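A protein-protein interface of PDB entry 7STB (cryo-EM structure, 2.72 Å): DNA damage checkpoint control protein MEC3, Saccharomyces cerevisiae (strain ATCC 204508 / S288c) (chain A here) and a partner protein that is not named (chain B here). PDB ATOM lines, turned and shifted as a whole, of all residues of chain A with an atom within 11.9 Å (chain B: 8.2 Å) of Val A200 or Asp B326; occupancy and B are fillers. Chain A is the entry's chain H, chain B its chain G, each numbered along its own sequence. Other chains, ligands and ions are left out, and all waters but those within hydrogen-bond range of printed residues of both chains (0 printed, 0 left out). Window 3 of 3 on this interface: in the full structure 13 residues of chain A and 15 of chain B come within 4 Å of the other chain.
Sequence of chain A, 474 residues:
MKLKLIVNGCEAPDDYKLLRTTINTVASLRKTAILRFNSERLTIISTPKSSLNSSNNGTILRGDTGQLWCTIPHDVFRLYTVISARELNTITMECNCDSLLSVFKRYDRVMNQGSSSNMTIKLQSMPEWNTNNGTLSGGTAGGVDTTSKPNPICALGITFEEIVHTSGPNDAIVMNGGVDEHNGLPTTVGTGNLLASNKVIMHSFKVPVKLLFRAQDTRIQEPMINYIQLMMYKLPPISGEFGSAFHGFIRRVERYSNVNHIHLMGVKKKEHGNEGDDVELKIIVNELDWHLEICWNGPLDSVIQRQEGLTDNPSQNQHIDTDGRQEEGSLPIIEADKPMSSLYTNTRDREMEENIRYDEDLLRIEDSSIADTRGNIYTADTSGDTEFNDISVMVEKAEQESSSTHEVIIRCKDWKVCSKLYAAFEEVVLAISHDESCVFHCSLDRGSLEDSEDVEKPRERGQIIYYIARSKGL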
ATOM      1  N   ARG A 106     -26.606  24.397  27.757  1.00  0.00           N
ATOM      2  CA  ARG A 106     -26.660  24.597  26.311  1.00  0.00           C
ATOM      3  C   ARG A 106     -27.484  25.834  25.971  1.00  0.00           C
ATOM      4  O   ARG A 106     -27.062  26.680  25.172  1.00  0.00           O
ATOM      5  CB  ARG A 106     -27.244  23.348  25.648  1.00  0.00           C
ATOM      6  CG  ARG A 106     -27.417  23.385  24.125  1.00  0.00           C
ATOM      7  CD  ARG A 106     -26.113  23.343  23.330  1.00  0.00           C
ATOM      8  NE  ARG A 106     -25.495  24.648  23.129  1.00  0.00           N
ATOM      9  CZ  ARG A 106     -24.290  24.827  22.605  1.00  0.00           C
ATOM     10  NH1 ARG A 106     -23.524  23.803  22.265  1.00  0.00           N
ATOM     11  NH2 ARG A 106     -23.844  26.064  22.406  1.00  0.00           N
ATOM     12  N   TYR A 107     -28.657  25.967  26.594  1.00  0.00           N
ATOM     13  CA  TYR A 107     -29.504  27.128  26.334  1.00  0.00           C
ATOM     14  C   TYR A 107     -28.837  28.418  26.799  1.00  0.00           C
ATOM     15  O   TYR A 107     -28.927  29.448  26.123  1.00  0.00           O
ATOM     16  CB  TYR A 107     -30.861  26.951  27.017  1.00  0.00           C
ATOM     17  CG  TYR A 107     -31.859  28.038  26.678  1.00  0.00           C
ATOM     18  CD1 TYR A 107     -32.135  28.367  25.359  1.00  0.00           C
ATOM     19  CD2 TYR A 107     -32.522  28.735  27.679  1.00  0.00           C
ATOM     20  CE1 TYR A 107     -33.042  29.359  25.044  1.00  0.00           C
ATOM     21  CE2 TYR A 107     -33.432  29.729  27.374  1.00  0.00           C
ATOM     22  CZ  TYR A 107     -33.688  30.036  26.054  1.00  0.00           C
ATOM     23  OH  TYR A 107     -34.594  31.024  25.745  1.00  0.00           O
ATOM     24  N   VAL A 110     -26.208  29.355  24.331  1.00  0.00           N
ATOM     25  CA  VAL A 110     -26.854  29.806  23.101  1.00  0.00           C
ATOM     26  C   VAL A 110     -27.327  31.247  23.255  1.00  0.00           C
ATOM     27  O   VAL A 110     -27.136  32.082  22.362  1.00  0.00           O
ATOM     28  CB  VAL A 110     -28.016  28.867  22.731  1.00  0.00           C
ATOM     29  CG1 VAL A 110     -28.944  29.531  21.720  1.00  0.00           C
ATOM     30  CG2 VAL A 110     -27.481  27.550  22.189  1.00  0.00           C
ATOM     31  N   GLN A 113     -24.399  33.649  23.212  1.00  0.00           N
ATOM     32  CA  GLN A 113     -23.985  33.925  21.842  1.00  0.00           C
ATOM     33  C   GLN A 113     -24.851  34.999  21.195  1.00  0.00           C
ATOM     34  O   GLN A 113     -24.411  35.640  20.235  1.00  0.00           O
ATOM     35  CB  GLN A 113     -24.033  32.641  21.012  1.00  0.00           C
ATOM     36  CG  GLN A 113     -23.550  32.801  19.577  1.00  0.00           C
ATOM     37  CD  GLN A 113     -22.097  33.224  19.494  1.00  0.00           C
ATOM     38  OE1 GLN A 113     -21.790  34.382  19.206  1.00  0.00           O
ATOM     39  NE2 GLN A 113     -21.191  32.286  19.747  1.00  0.00           N
ATOM     40  N   GLY A 114     -26.065  35.207  21.698  1.00  0.00           N
ATOM     41  CA  GLY A 114     -26.946  36.235  21.181  1.00  0.00           C
ATOM     42  C   GLY A 114     -28.049  35.680  20.304  1.00  0.00           C
ATOM     43  O   GLY A 114     -27.826  35.385  19.126  1.00  0.00           O
ATOM     44  N   SER A 115     -29.243  35.534  20.869  1.00  0.00           N
ATOM     45  CA  SER A 115     -30.387  35.024  20.126  1.00  0.00           C
ATOM     46  C   SER A 115     -31.650  35.306  20.924  1.00  0.00           C
ATOM     47  O   SER A 115     -31.604  35.506  22.141  1.00  0.00           O
ATOM     48  CB  SER A 115     -30.253  33.523  19.846  1.00  0.00           C
ATOM     49  OG  SER A 115     -30.450  32.766  21.026  1.00  0.00           O
ATOM     50  N   SER A 116     -32.781  35.320  20.217  1.00  0.00           N
ATOM     51  CA  SER A 116     -34.091  35.524  20.823  1.00  0.00           C
ATOM     52  C   SER A 116     -34.935  34.255  20.799  1.00  0.00           C
ATOM     53  O   SER A 116     -36.164  34.327  20.905  1.00  0.00           O
ATOM     54  CB  SER A 116     -34.827  36.663  20.115  1.00  0.00           C
ATOM     55  OG  SER A 116     -34.146  37.894  20.286  1.00  0.00           O
ATOM     56  N   SER A 117     -34.301  33.094  20.663  1.00  0.00           N
ATOM     57  CA  SER A 117     -35.035  31.841  20.584  1.00  0.00           C
ATOM     58  C   SER A 117     -35.702  31.520  21.917  1.00  0.00           C
ATOM     59  O   SER A 117     -35.247  31.937  22.986  1.00  0.00           O
ATOM     60  CB  SER A 117     -34.099  30.700  20.183  1.00  0.00           C
ATOM     61  OG  SER A 117     -33.099  30.493  21.165  1.00  0.00           O
ATOM     62  N   ASN A 118     -36.796  30.768  21.842  1.00  0.00           N
ATOM     63  CA  ASN A 118     -37.562  30.359  23.009  1.00  0.00           C
ATOM     64  C   ASN A 118     -37.409  28.861  23.226  1.00  0.00           C
ATOM     65  O   ASN A 118     -37.403  28.082  22.268  1.00  0.00           O
ATOM     66  CB  ASN A 118     -39.044  30.708  22.842  1.00  0.00           C
ATOM     67  CG  ASN A 118     -39.262  32.138  22.394  1.00  0.00           C
ATOM     68  OD1 ASN A 118     -39.535  33.020  23.206  1.00  0.00           O
ATOM     69  ND2 ASN A 118     -39.141  32.374  21.092  1.00  0.00           N
ATOM     70  N   THR A 159     -36.899  21.818  23.274  1.00  0.00           N
ATOM     71  CA  THR A 159     -36.477  22.240  21.946  1.00  0.00           C
ATOM     72  C   THR A 159     -36.266  23.745  21.922  1.00  0.00           C
ATOM     73  O   THR A 159     -37.116  24.503  22.401  1.00  0.00           O
ATOM     74  CB  THR A 159     -37.510  21.842  20.887  1.00  0.00           C
ATOM     75  OG1 THR A 159     -38.804  22.326  21.268  1.00  0.00           O
ATOM     76  CG2 THR A 159     -37.562  20.331  20.727  1.00  0.00           C
ATOM     77  N   PHE A 160     -35.135  24.172  21.363  1.00  0.00           N
ATOM     78  CA  PHE A 160     -34.883  25.589  21.133  1.00  0.00           C
ATOM     79  C   PHE A 160     -33.954  25.739  19.941  1.00  0.00           C
ATOM     80  O   PHE A 160     -33.237  24.809  19.568  1.00  0.00           O
ATOM     81  CB  PHE A 160     -34.287  26.278  22.368  1.00  0.00           C
ATOM     82  CG  PHE A 160     -33.058  25.610  22.913  1.00  0.00           C
ATOM     83  CD1 PHE A 160     -31.810  25.882  22.379  1.00  0.00           C
ATOM     84  CD2 PHE A 160     -33.148  24.726  23.974  1.00  0.00           C
ATOM     85  CE1 PHE A 160     -30.678  25.275  22.884  1.00  0.00           C
ATOM     86  CE2 PHE A 160     -32.020  24.117  24.484  1.00  0.00           C
ATOM     87  CZ  PHE A 160     -30.783  24.391  23.938  1.00  0.00           C
ATOM     88  N   GLU A 161     -33.972  26.927  19.347  1.00  0.00           N
ATOM     89  CA  GLU A 161     -33.182  27.224  18.162  1.00  0.00           C
ATOM     90  C   GLU A 161     -31.893  27.947  18.543  1.00  0.00           C
ATOM     91  O   GLU A 161     -31.672  28.323  19.695  1.00  0.00           O
ATOM     92  CB  GLU A 161     -33.994  28.067  17.175  1.00  0.00           C
ATOM     93  CG  GLU A 161     -35.175  27.334  16.563  1.00  0.00           C
ATOM     94  CD  GLU A 161     -35.969  28.200  15.606  1.00  0.00           C
ATOM     95  OE1 GLU A 161     -35.674  29.410  15.514  1.00  0.00           O
ATOM     96  OE2 GLU A 161     -36.887  27.672  14.946  1.00  0.00           O
ATOM     97  N   GLU A 162     -31.033  28.136  17.542  1.00  0.00           N
ATOM     98  CA  GLU A 162     -29.755  28.814  17.748  1.00  0.00           C
ATOM     99  C   GLU A 162     -29.324  29.410  16.415  1.00  0.00           C
ATOM    100  O   GLU A 162     -28.984  28.666  15.489  1.00  0.00           O
ATOM    101  CB  GLU A 162     -28.705  27.847  18.284  1.00  0.00           C
ATOM    102  CG  GLU A 162     -27.349  28.486  18.564  1.00  0.00           C
ATOM    103  CD  GLU A 162     -26.223  27.472  18.617  1.00  0.00           C
ATOM    104  OE1 GLU A 162     -26.201  26.557  17.765  1.00  0.00           O
ATOM    105  OE2 GLU A 162     -25.356  27.588  19.508  1.00  0.00           O
ATOM    106  N   ILE A 163     -29.335  30.736  16.321  1.00  0.00           N
ATOM    107  CA  ILE A 163     -28.913  31.418  15.106  1.00  0.00           C
ATOM    108  C   ILE A 163     -27.420  31.713  15.185  1.00  0.00           C
ATOM    109  O   ILE A 163     -26.709  31.148  16.018  1.00  0.00           O
ATOM    110  CB  ILE A 163     -29.719  32.709  14.881  1.00  0.00           C
ATOM    111  CG1 ILE A 163     -31.217  32.426  15.031  1.00  0.00           C
ATOM    112  CG2 ILE A 163     -29.418  33.292  13.504  1.00  0.00           C
ATOM    113  CD1 ILE A 163     -32.115  33.543  14.537  1.00  0.00           C
ATOM    114  N   VAL A 200     -29.593  28.731  11.185  1.00  0.00           N
ATOM    115  CA  VAL A 200     -30.320  28.269  12.360  1.00  0.00           C
ATOM    116  C   VAL A 200     -30.088  26.778  12.564  1.00  0.00           C
ATOM    117  O   VAL A 200     -30.105  26.001  11.610  1.00  0.00           O
ATOM    118  CB  VAL A 200     -31.825  28.574  12.239  1.00  0.00           C
ATOM    119  CG1 VAL A 200     -32.406  27.932  10.986  1.00  0.00           C
ATOM    120  CG2 VAL A 200     -32.565  28.098  13.482  1.00  0.00           C
ATOM    121  N   ILE A 201     -29.872  26.385  13.816  1.00  0.00           N
ATOM    122  CA  ILE A 201     -29.656  24.992  14.189  1.00  0.00           C
ATOM    123  C   ILE A 201     -30.716  24.617  15.213  1.00  0.00           C
ATOM    124  O   ILE A 201     -30.851  25.284  16.246  1.00  0.00           O
ATOM    125  CB  ILE A 201     -28.244  24.760  14.750  1.00  0.00           C
ATOM    126  CG1 ILE A 201     -27.189  25.224  13.742  1.00  0.00           C
ATOM    127  CG2 ILE A 201     -28.044  23.288  15.096  1.00  0.00           C
ATOM    128  CD1 ILE A 201     -25.772  25.172  14.267  1.00  0.00           C
ATOM    129  N   MET A 202     -31.462  23.552  14.931  1.00  0.00           N
ATOM    130  CA  MET A 202     -32.492  23.086  15.847  1.00  0.00           C
ATOM    131  C   MET A 202     -31.867  22.204  16.919  1.00  0.00           C
ATOM    132  O   MET A 202     -31.239  21.188  16.611  1.00  0.00           O
ATOM    133  CB  MET A 202     -33.570  22.311  15.089  1.00  0.00           C
ATOM    134  CG  MET A 202     -34.567  23.189  14.353  1.00  0.00           C
ATOM    135  SD  MET A 202     -33.921  23.819  12.793  1.00  0.00           S
ATOM    136  CE  MET A 202     -34.049  22.361  11.760  1.00  0.00           C
ATOM    137  N   HIS A 203     -32.044  22.595  18.176  1.00  0.00           N
ATOM    138  CA  HIS A 203     -31.559  21.839  19.323  1.00  0.00           C
ATOM    139  C   HIS A 203     -32.745  21.145  19.976  1.00  0.00           C
ATOM    140  O   HIS A 203     -33.699  21.809  20.399  1.00  0.00           O
ATOM    141  CB  HIS A 203     -30.854  22.751  20.328  1.00  0.00           C
ATOM    142  CG  HIS A 203     -29.574  23.336  19.820  1.00  0.00           C
ATOM    143  ND1 HIS A 203     -29.509  24.113  18.683  1.00  0.00           N
ATOM    144  CD2 HIS A 203     -28.309  23.264  20.298  1.00  0.00           C
ATOM    145  CE1 HIS A 203     -28.260  24.490  18.480  1.00  0.00           C
ATOM    146  NE2 HIS A 203     -27.512  23.988  19.446  1.00  0.00           N
ATOM    147  N   SER A 204     -32.682  19.817  20.053  1.00  0.00           N
ATOM    148  CA  SER A 204     -33.741  19.003  20.632  1.00  0.00           C
ATOM    149  C   SER A 204     -33.140  18.040  21.645  1.00  0.00           C
ATOM    150  O   SER A 204     -32.054  17.497  21.428  1.00  0.00           O
ATOM    151  CB  SER A 204     -34.495  18.223  19.549  1.00  0.00           C
ATOM    152  OG  SER A 204     -35.505  17.409  20.118  1.00  0.00           O
ATOM    153  N   CYS B 265     -19.922  16.491   3.067  1.00  0.00           N
ATOM    154  CA  CYS B 265     -18.899  17.444   3.481  1.00  0.00           C
ATOM    155  C   CYS B 265     -19.578  18.561   4.262  1.00  0.00           C
ATOM    156  O   CYS B 265     -20.448  19.257   3.725  1.00  0.00           O
ATOM    157  CB  CYS B 265     -18.150  18.010   2.277  1.00  0.00           C
ATOM    158  SG  CYS B 265     -16.854  19.195   2.700  1.00  0.00           S
ATOM    159  N   CYS B 266     -19.180  18.732   5.523  1.00  0.00           N
ATOM    160  CA  CYS B 266     -19.847  19.662   6.423  1.00  0.00           C
ATOM    161  C   CYS B 266     -18.823  20.501   7.174  1.00  0.00           C
ATOM    162  O   CYS B 266     -17.731  20.032   7.505  1.00  0.00           O
ATOM    163  CB  CYS B 266     -20.739  18.916   7.425  1.00  0.00           C
ATOM    164  SG  CYS B 266     -21.602  19.984   8.597  1.00  0.00           S
ATOM    165  N   ASN B 267     -19.196  21.747   7.455  1.00  0.00           N
ATOM    166  CA  ASN B 267     -18.330  22.632   8.224  1.00  0.00           C
ATOM    167  C   ASN B 267     -18.112  22.061   9.618  1.00  0.00           C
ATOM    168  O   ASN B 267     -19.071  21.795  10.349  1.00  0.00           O
ATOM    169  CB  ASN B 267     -18.947  24.027   8.307  1.00  0.00           C
ATOM    170  CG  ASN B 267     -17.916  25.105   8.577  1.00  0.00           C
ATOM    171  OD1 ASN B 267     -17.541  25.346   9.725  1.00  0.00           O
ATOM    172  ND2 ASN B 267     -17.450  25.757   7.519  1.00  0.00           N
ATOM    173  N   LEU B 270     -19.993  23.289  13.335  1.00  0.00           N
ATOM    174  CA  LEU B 270     -21.263  22.851  13.909  1.00  0.00           C
ATOM    175  C   LEU B 270     -21.113  21.513  14.622  1.00  0.00           C
ATOM    176  O   LEU B 270     -21.549  21.350  15.769  1.00  0.00           O
ATOM    177  CB  LEU B 270     -22.323  22.753  12.812  1.00  0.00           C
ATOM    178  CG  LEU B 270     -22.942  24.067  12.331  1.00  0.00           C
ATOM    179  CD1 LEU B 270     -21.947  24.873  11.510  1.00  0.00           C
ATOM    180  CD2 LEU B 270     -24.203  23.793  11.528  1.00  0.00           C
ATOM    181  N   HIS B 293     -33.756  17.007   2.568  1.00  0.00           N
ATOM    182  CA  HIS B 293     -34.075  18.322   3.104  1.00  0.00           C
ATOM    183  C   HIS B 293     -33.291  18.694   4.352  1.00  0.00           C
ATOM    184  O   HIS B 293     -33.090  19.886   4.596  1.00  0.00           O
ATOM    185  CB  HIS B 293     -35.574  18.413   3.433  1.00  0.00           C
ATOM    186  CG  HIS B 293     -36.469  18.136   2.265  1.00  0.00           C
ATOM    187  ND1 HIS B 293     -36.518  18.952   1.156  1.00  0.00           N
ATOM    188  CD2 HIS B 293     -37.352  17.136   2.036  1.00  0.00           C
ATOM    189  CE1 HIS B 293     -37.392  18.465   0.293  1.00  0.00           C
ATOM    190  NE2 HIS B 293     -37.911  17.363   0.803  1.00  0.00           N
ATOM    191  N   LEU B 295     -30.270  17.334   7.664  1.00  0.00           N
ATOM    192  CA  LEU B 295     -29.314  16.423   8.277  1.00  0.00           C
ATOM    193  C   LEU B 295     -29.451  16.524   9.788  1.00  0.00           C
ATOM    194  O   LEU B 295     -29.418  17.626  10.344  1.00  0.00           O
ATOM    195  CB  LEU B 295     -27.878  16.751   7.852  1.00  0.00           C
ATOM    196  CG  LEU B 295     -26.773  15.823   8.375  1.00  0.00           C
ATOM    197  CD1 LEU B 295     -25.565  15.844   7.452  1.00  0.00           C
ATOM    198  CD2 LEU B 295     -26.350  16.189   9.794  1.00  0.00           C
ATOM    199  N   THR B 321     -30.377  19.306  14.394  1.00  0.00           N
ATOM    200  CA  THR B 321     -30.827  19.193  13.015  1.00  0.00           C
ATOM    201  C   THR B 321     -30.556  20.497  12.278  1.00  0.00           C
ATOM    202  O   THR B 321     -30.759  21.585  12.826  1.00  0.00           O
ATOM    203  CB  THR B 321     -32.322  18.861  12.947  1.00  0.00           C
ATOM    204  OG1 THR B 321     -32.589  17.681  13.713  1.00  0.00           O
ATOM    205  CG2 THR B 321     -32.760  18.638  11.508  1.00  0.00           C
ATOM    206  N   ILE B 322     -30.092  20.379  11.033  1.00  0.00           N
ATOM    207  CA  ILE B 322     -29.832  21.530  10.179  1.00  0.00           C
ATOM    208  C   ILE B 322     -30.354  21.230   8.781  1.00  0.00           C
ATOM    209  O   ILE B 322     -30.645  20.085   8.434  1.00  0.00           O
ATOM    210  CB  ILE B 322     -28.330  21.895  10.132  1.00  0.00           C
ATOM    211  CG1 ILE B 322     -27.506  20.746   9.544  1.00  0.00           C
ATOM    212  CG2 ILE B 322     -27.832  22.247  11.524  1.00  0.00           C
ATOM    213  CD1 ILE B 322     -26.069  21.114   9.253  1.00  0.00           C
ATOM    214  N   SER B 323     -30.487  22.281   7.980  1.00  0.00           N
ATOM    215  CA  SER B 323     -30.927  22.125   6.604  1.00  0.00           C
ATOM    216  C   SER B 323     -29.760  21.715   5.715  1.00  0.00           C
ATOM    217  O   SER B 323     -28.595  21.990   6.016  1.00  0.00           O
ATOM    218  CB  SER B 323     -31.545  23.424   6.085  1.00  0.00           C
ATOM    219  OG  SER B 323     -30.564  24.438   5.954  1.00  0.00           O
ATOM    220  N   THR B 324     -30.084  21.045   4.608  1.00  0.00           N
ATOM    221  CA  THR B 324     -29.053  20.632   3.663  1.00  0.00           C
ATOM    222  C   THR B 324     -28.365  21.820   3.006  1.00  0.00           C
ATOM    223  O   THR B 324     -27.248  21.670   2.499  1.00  0.00           O
ATOM    224  CB  THR B 324     -29.651  19.726   2.585  1.00  0.00           C
ATOM    225  OG1 THR B 324     -30.814  20.347   2.024  1.00  0.00           O
ATOM    226  CG2 THR B 324     -30.025  18.374   3.171  1.00  0.00           C
ATOM    227  N   LEU B 325     -29.002  22.994   3.000  1.00  0.00           N
ATOM    228  CA  LEU B 325     -28.352  24.177   2.448  1.00  0.00           C
ATOM    229  C   LEU B 325     -27.156  24.598   3.291  1.00  0.00           C
ATOM    230  O   LEU B 325     -26.183  25.142   2.755  1.00  0.00           O
ATOM    231  CB  LEU B 325     -29.356  25.323   2.340  1.00  0.00           C
ATOM    232  CG  LEU B 325     -30.666  24.992   1.621  1.00  0.00           C
ATOM    233  CD1 LEU B 325     -31.570  26.214   1.565  1.00  0.00           C
ATOM    234  CD2 LEU B 325     -30.397  24.458   0.221  1.00  0.00           C
ATOM    235  N   ASP B 326     -27.207  24.359   4.604  1.00  0.00           N
ATOM    236  CA  ASP B 326     -26.067  24.670   5.457  1.00  0.00           C
ATOM    237  C   ASP B 326     -24.871  23.780   5.140  1.00  0.00           C
ATOM    238  O   ASP B 326     -23.724  24.236   5.213  1.00  0.00           O
ATOM    239  CB  ASP B 326     -26.456  24.523   6.927  1.00  0.00           C
ATOM    240  CG  ASP B 326     -27.540  25.498   7.341  1.00  0.00           C
ATOM    241  OD1 ASP B 326     -27.836  26.428   6.562  1.00  0.00           O
ATOM    242  OD2 ASP B 326     -28.097  25.335   8.448  1.00  0.00           O
ATOM    243  N   LEU B 327     -25.116  22.520   4.788  1.00  0.00           N
ATOM    244  CA  LEU B 327     -24.029  21.603   4.475  1.00  0.00           C
ATOM    245  C   LEU B 327     -23.249  22.090   3.262  1.00  0.00           C
ATOM    246  O   LEU B 327     -23.813  22.672   2.331  1.00  0.00           O
ATOM    247  CB  LEU B 327     -24.580  20.203   4.208  1.00  0.00           C
ATOM    248  CG  LEU B 327     -25.299  19.515   5.368  1.00  0.00           C
ATOM    249  CD1 LEU B 327     -25.759  18.132   4.945  1.00  0.00           C
ATOM    250  CD2 LEU B 327     -24.402  19.431   6.590  1.00  0.00           C
ATOM    251  N   GLU B 328     -21.937  21.851   3.278  1.00  0.00           N
ATOM    252  CA  GLU B 328     -21.107  22.232   2.141  1.00  0.00           C
ATOM    253  C   GLU B 328     -21.427  21.376   0.921  1.00  0.00           C
ATOM    254  O   GLU B 328     -21.624  21.899  -0.181  1.00  0.00           O
ATOM    255  CB  GLU B 328     -19.627  22.119   2.513  1.00  0.00           C
ATOM    256  CG  GLU B 328     -18.672  22.537   1.408  1.00  0.00           C
ATOM    257  CD  GLU B 328     -18.785  24.010   1.067  1.00  0.00           C
ATOM    258  OE1 GLU B 328     -19.200  24.795   1.944  1.00  0.00           O
ATOM    259  OE2 GLU B 328     -18.459  24.382  -0.081  1.00  0.00           O
ATOM    260  N   HIS B 329     -21.486  20.056   1.098  1.00  0.00           N
ATOM    261  CA  HIS B 329     -21.827  19.157   0.004  1.00  0.00           C
ATOM    262  C   HIS B 329     -22.532  17.931   0.561  1.00  0.00           C
ATOM    263  O   HIS B 329     -22.240  17.482   1.670  1.00  0.00           O
ATOM    264  CB  HIS B 329     -20.588  18.716  -0.786  1.00  0.00           C
ATOM    265  CG  HIS B 329     -19.908  19.828  -1.522  1.00  0.00           C
ATOM    266  ND1 HIS B 329     -18.615  20.217  -1.250  1.00  0.00           N
ATOM    267  CD2 HIS B 329     -20.340  20.628  -2.525  1.00  0.00           C
ATOM    268  CE1 HIS B 329     -18.280  21.212  -2.052  1.00  0.00           C
ATOM    269  NE2 HIS B 329     -19.308  21.481  -2.835  1.00  0.00           N
ATOM    270  N   TYR B 330     -23.449  17.379  -0.232  1.00  0.00           N
ATOM    271  CA  TYR B 330     -24.116  16.135   0.127  1.00  0.00           C
ATOM    272  C   TYR B 330     -24.446  15.365  -1.142  1.00  0.00           C
ATOM    273  O   TYR B 330     -24.937  15.946  -2.115  1.00  0.00           O
ATOM    274  CB  TYR B 330     -25.385  16.397   0.946  1.00  0.00           C
ATOM    275  CG  TYR B 330     -26.548  16.939   0.144  1.00  0.00           C
ATOM    276  CD1 TYR B 330     -26.659  18.295  -0.126  1.00  0.00           C
ATOM    277  CD2 TYR B 330     -27.539  16.093  -0.337  1.00  0.00           C
ATOM    278  CE1 TYR B 330     -27.720  18.795  -0.855  1.00  0.00           C
ATOM    279  CE2 TYR B 330     -28.604  16.583  -1.066  1.00  0.00           C
ATOM    280  CZ  TYR B 330     -28.690  17.934  -1.323  1.00  0.00           C
ATOM    281  OH  TYR B 330     -29.750  18.425  -2.050  1.00  0.00           O
ATOM    282  N   ASN B 382     -13.333  21.759   7.207  1.00  0.00           N
ATOM    283  CA  ASN B 382     -14.474  20.951   6.807  1.00  0.00           C
ATOM    284  C   ASN B 382     -14.153  19.479   7.023  1.00  0.00           C
ATOM    285  O   ASN B 382     -13.022  19.040   6.791  1.00  0.00           O
ATOM    286  CB  ASN B 382     -14.834  21.190   5.338  1.00  0.00           C
ATOM    287  CG  ASN B 382     -15.307  22.604   5.076  1.00  0.00           C
ATOM    288  OD1 ASN B 382     -16.224  23.095   5.731  1.00  0.00           O
ATOM    289  ND2 ASN B 382     -14.684  23.266   4.110  1.00  0.00           N
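Of chain B, only Asp B326 (3.8 Å) comes within 4 Å of Val A200. Of the printed residues of chain A, Asp B326 touches Val A200 (3.8 Å). No residue of chain A comes within 4 Å of Cys B266. Asn B267 touches none of the printed residues of chain A. Of chain A, only Ile A201 (3.7 Å) comes within 4 Å of Ile B322. Thr B324 touches none of the printed residues of chain A. No residue of chain A comes within 4 Å of Leu B325. Printed residues of chain B within 4 Å of Ile A201: Leu B270, Thr B321 and Ile B322. Of the printed residues of chain A, Leu B270 touches Ile A201. The nearest residue of chain B that does not touch Val A200 is Ile B322 (4.4 Å). The nearest residue of chain A that does not touch Asp B326 is Ile A201 (5.4 Å). The nearest printed residue of chain A that does not touch Thr B321 is Val A200 (4.6 Å).
Of the 19 printed residues of chain A, 3 touch a printed residue of chain B. Of the 17 printed residues of chain B, 4 touch a printed residue of chain A. Among the printed residues, 5 pairs touch across the chains. Among the printed residues, no Asp or Glu carboxylate lies within 4 Å of a Lys or Arg side-chain nitrogen of the other chain.
Among the printed residues, pairs that only touch across the chains: Val A200 with Asp B326 (3.8 Å), Ile A201 with Leu B270 (3.4 Å), Ile A201 with Thr B321 (3.8 Å) and Ile A201 with Ile B322 (3.7 Å).
O of Thr B321 is in hydrogen-bond range of N of Met A202 (3.0 Å).
The backbone carbonyl oxygen (O) of Ile B322 sits at hydrogen-bond distance from the backbone NH (N) of Leu B295 (2.9 Å). OG of Ser B323 is in hydrogen-bond range of OD1 of Asp B326, 3.4 Å away. The backbone carbonyl oxygen (O) of Glu A162 lies within hydrogen-bond range of the backbone NH (N) of Ile A201 (3.0 Å). A ring nitrogen (ND1) of His A203 lies within hydrogen-bond range of the backbone carbonyl oxygen (O) of Ile A201, at 3.0 Å.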
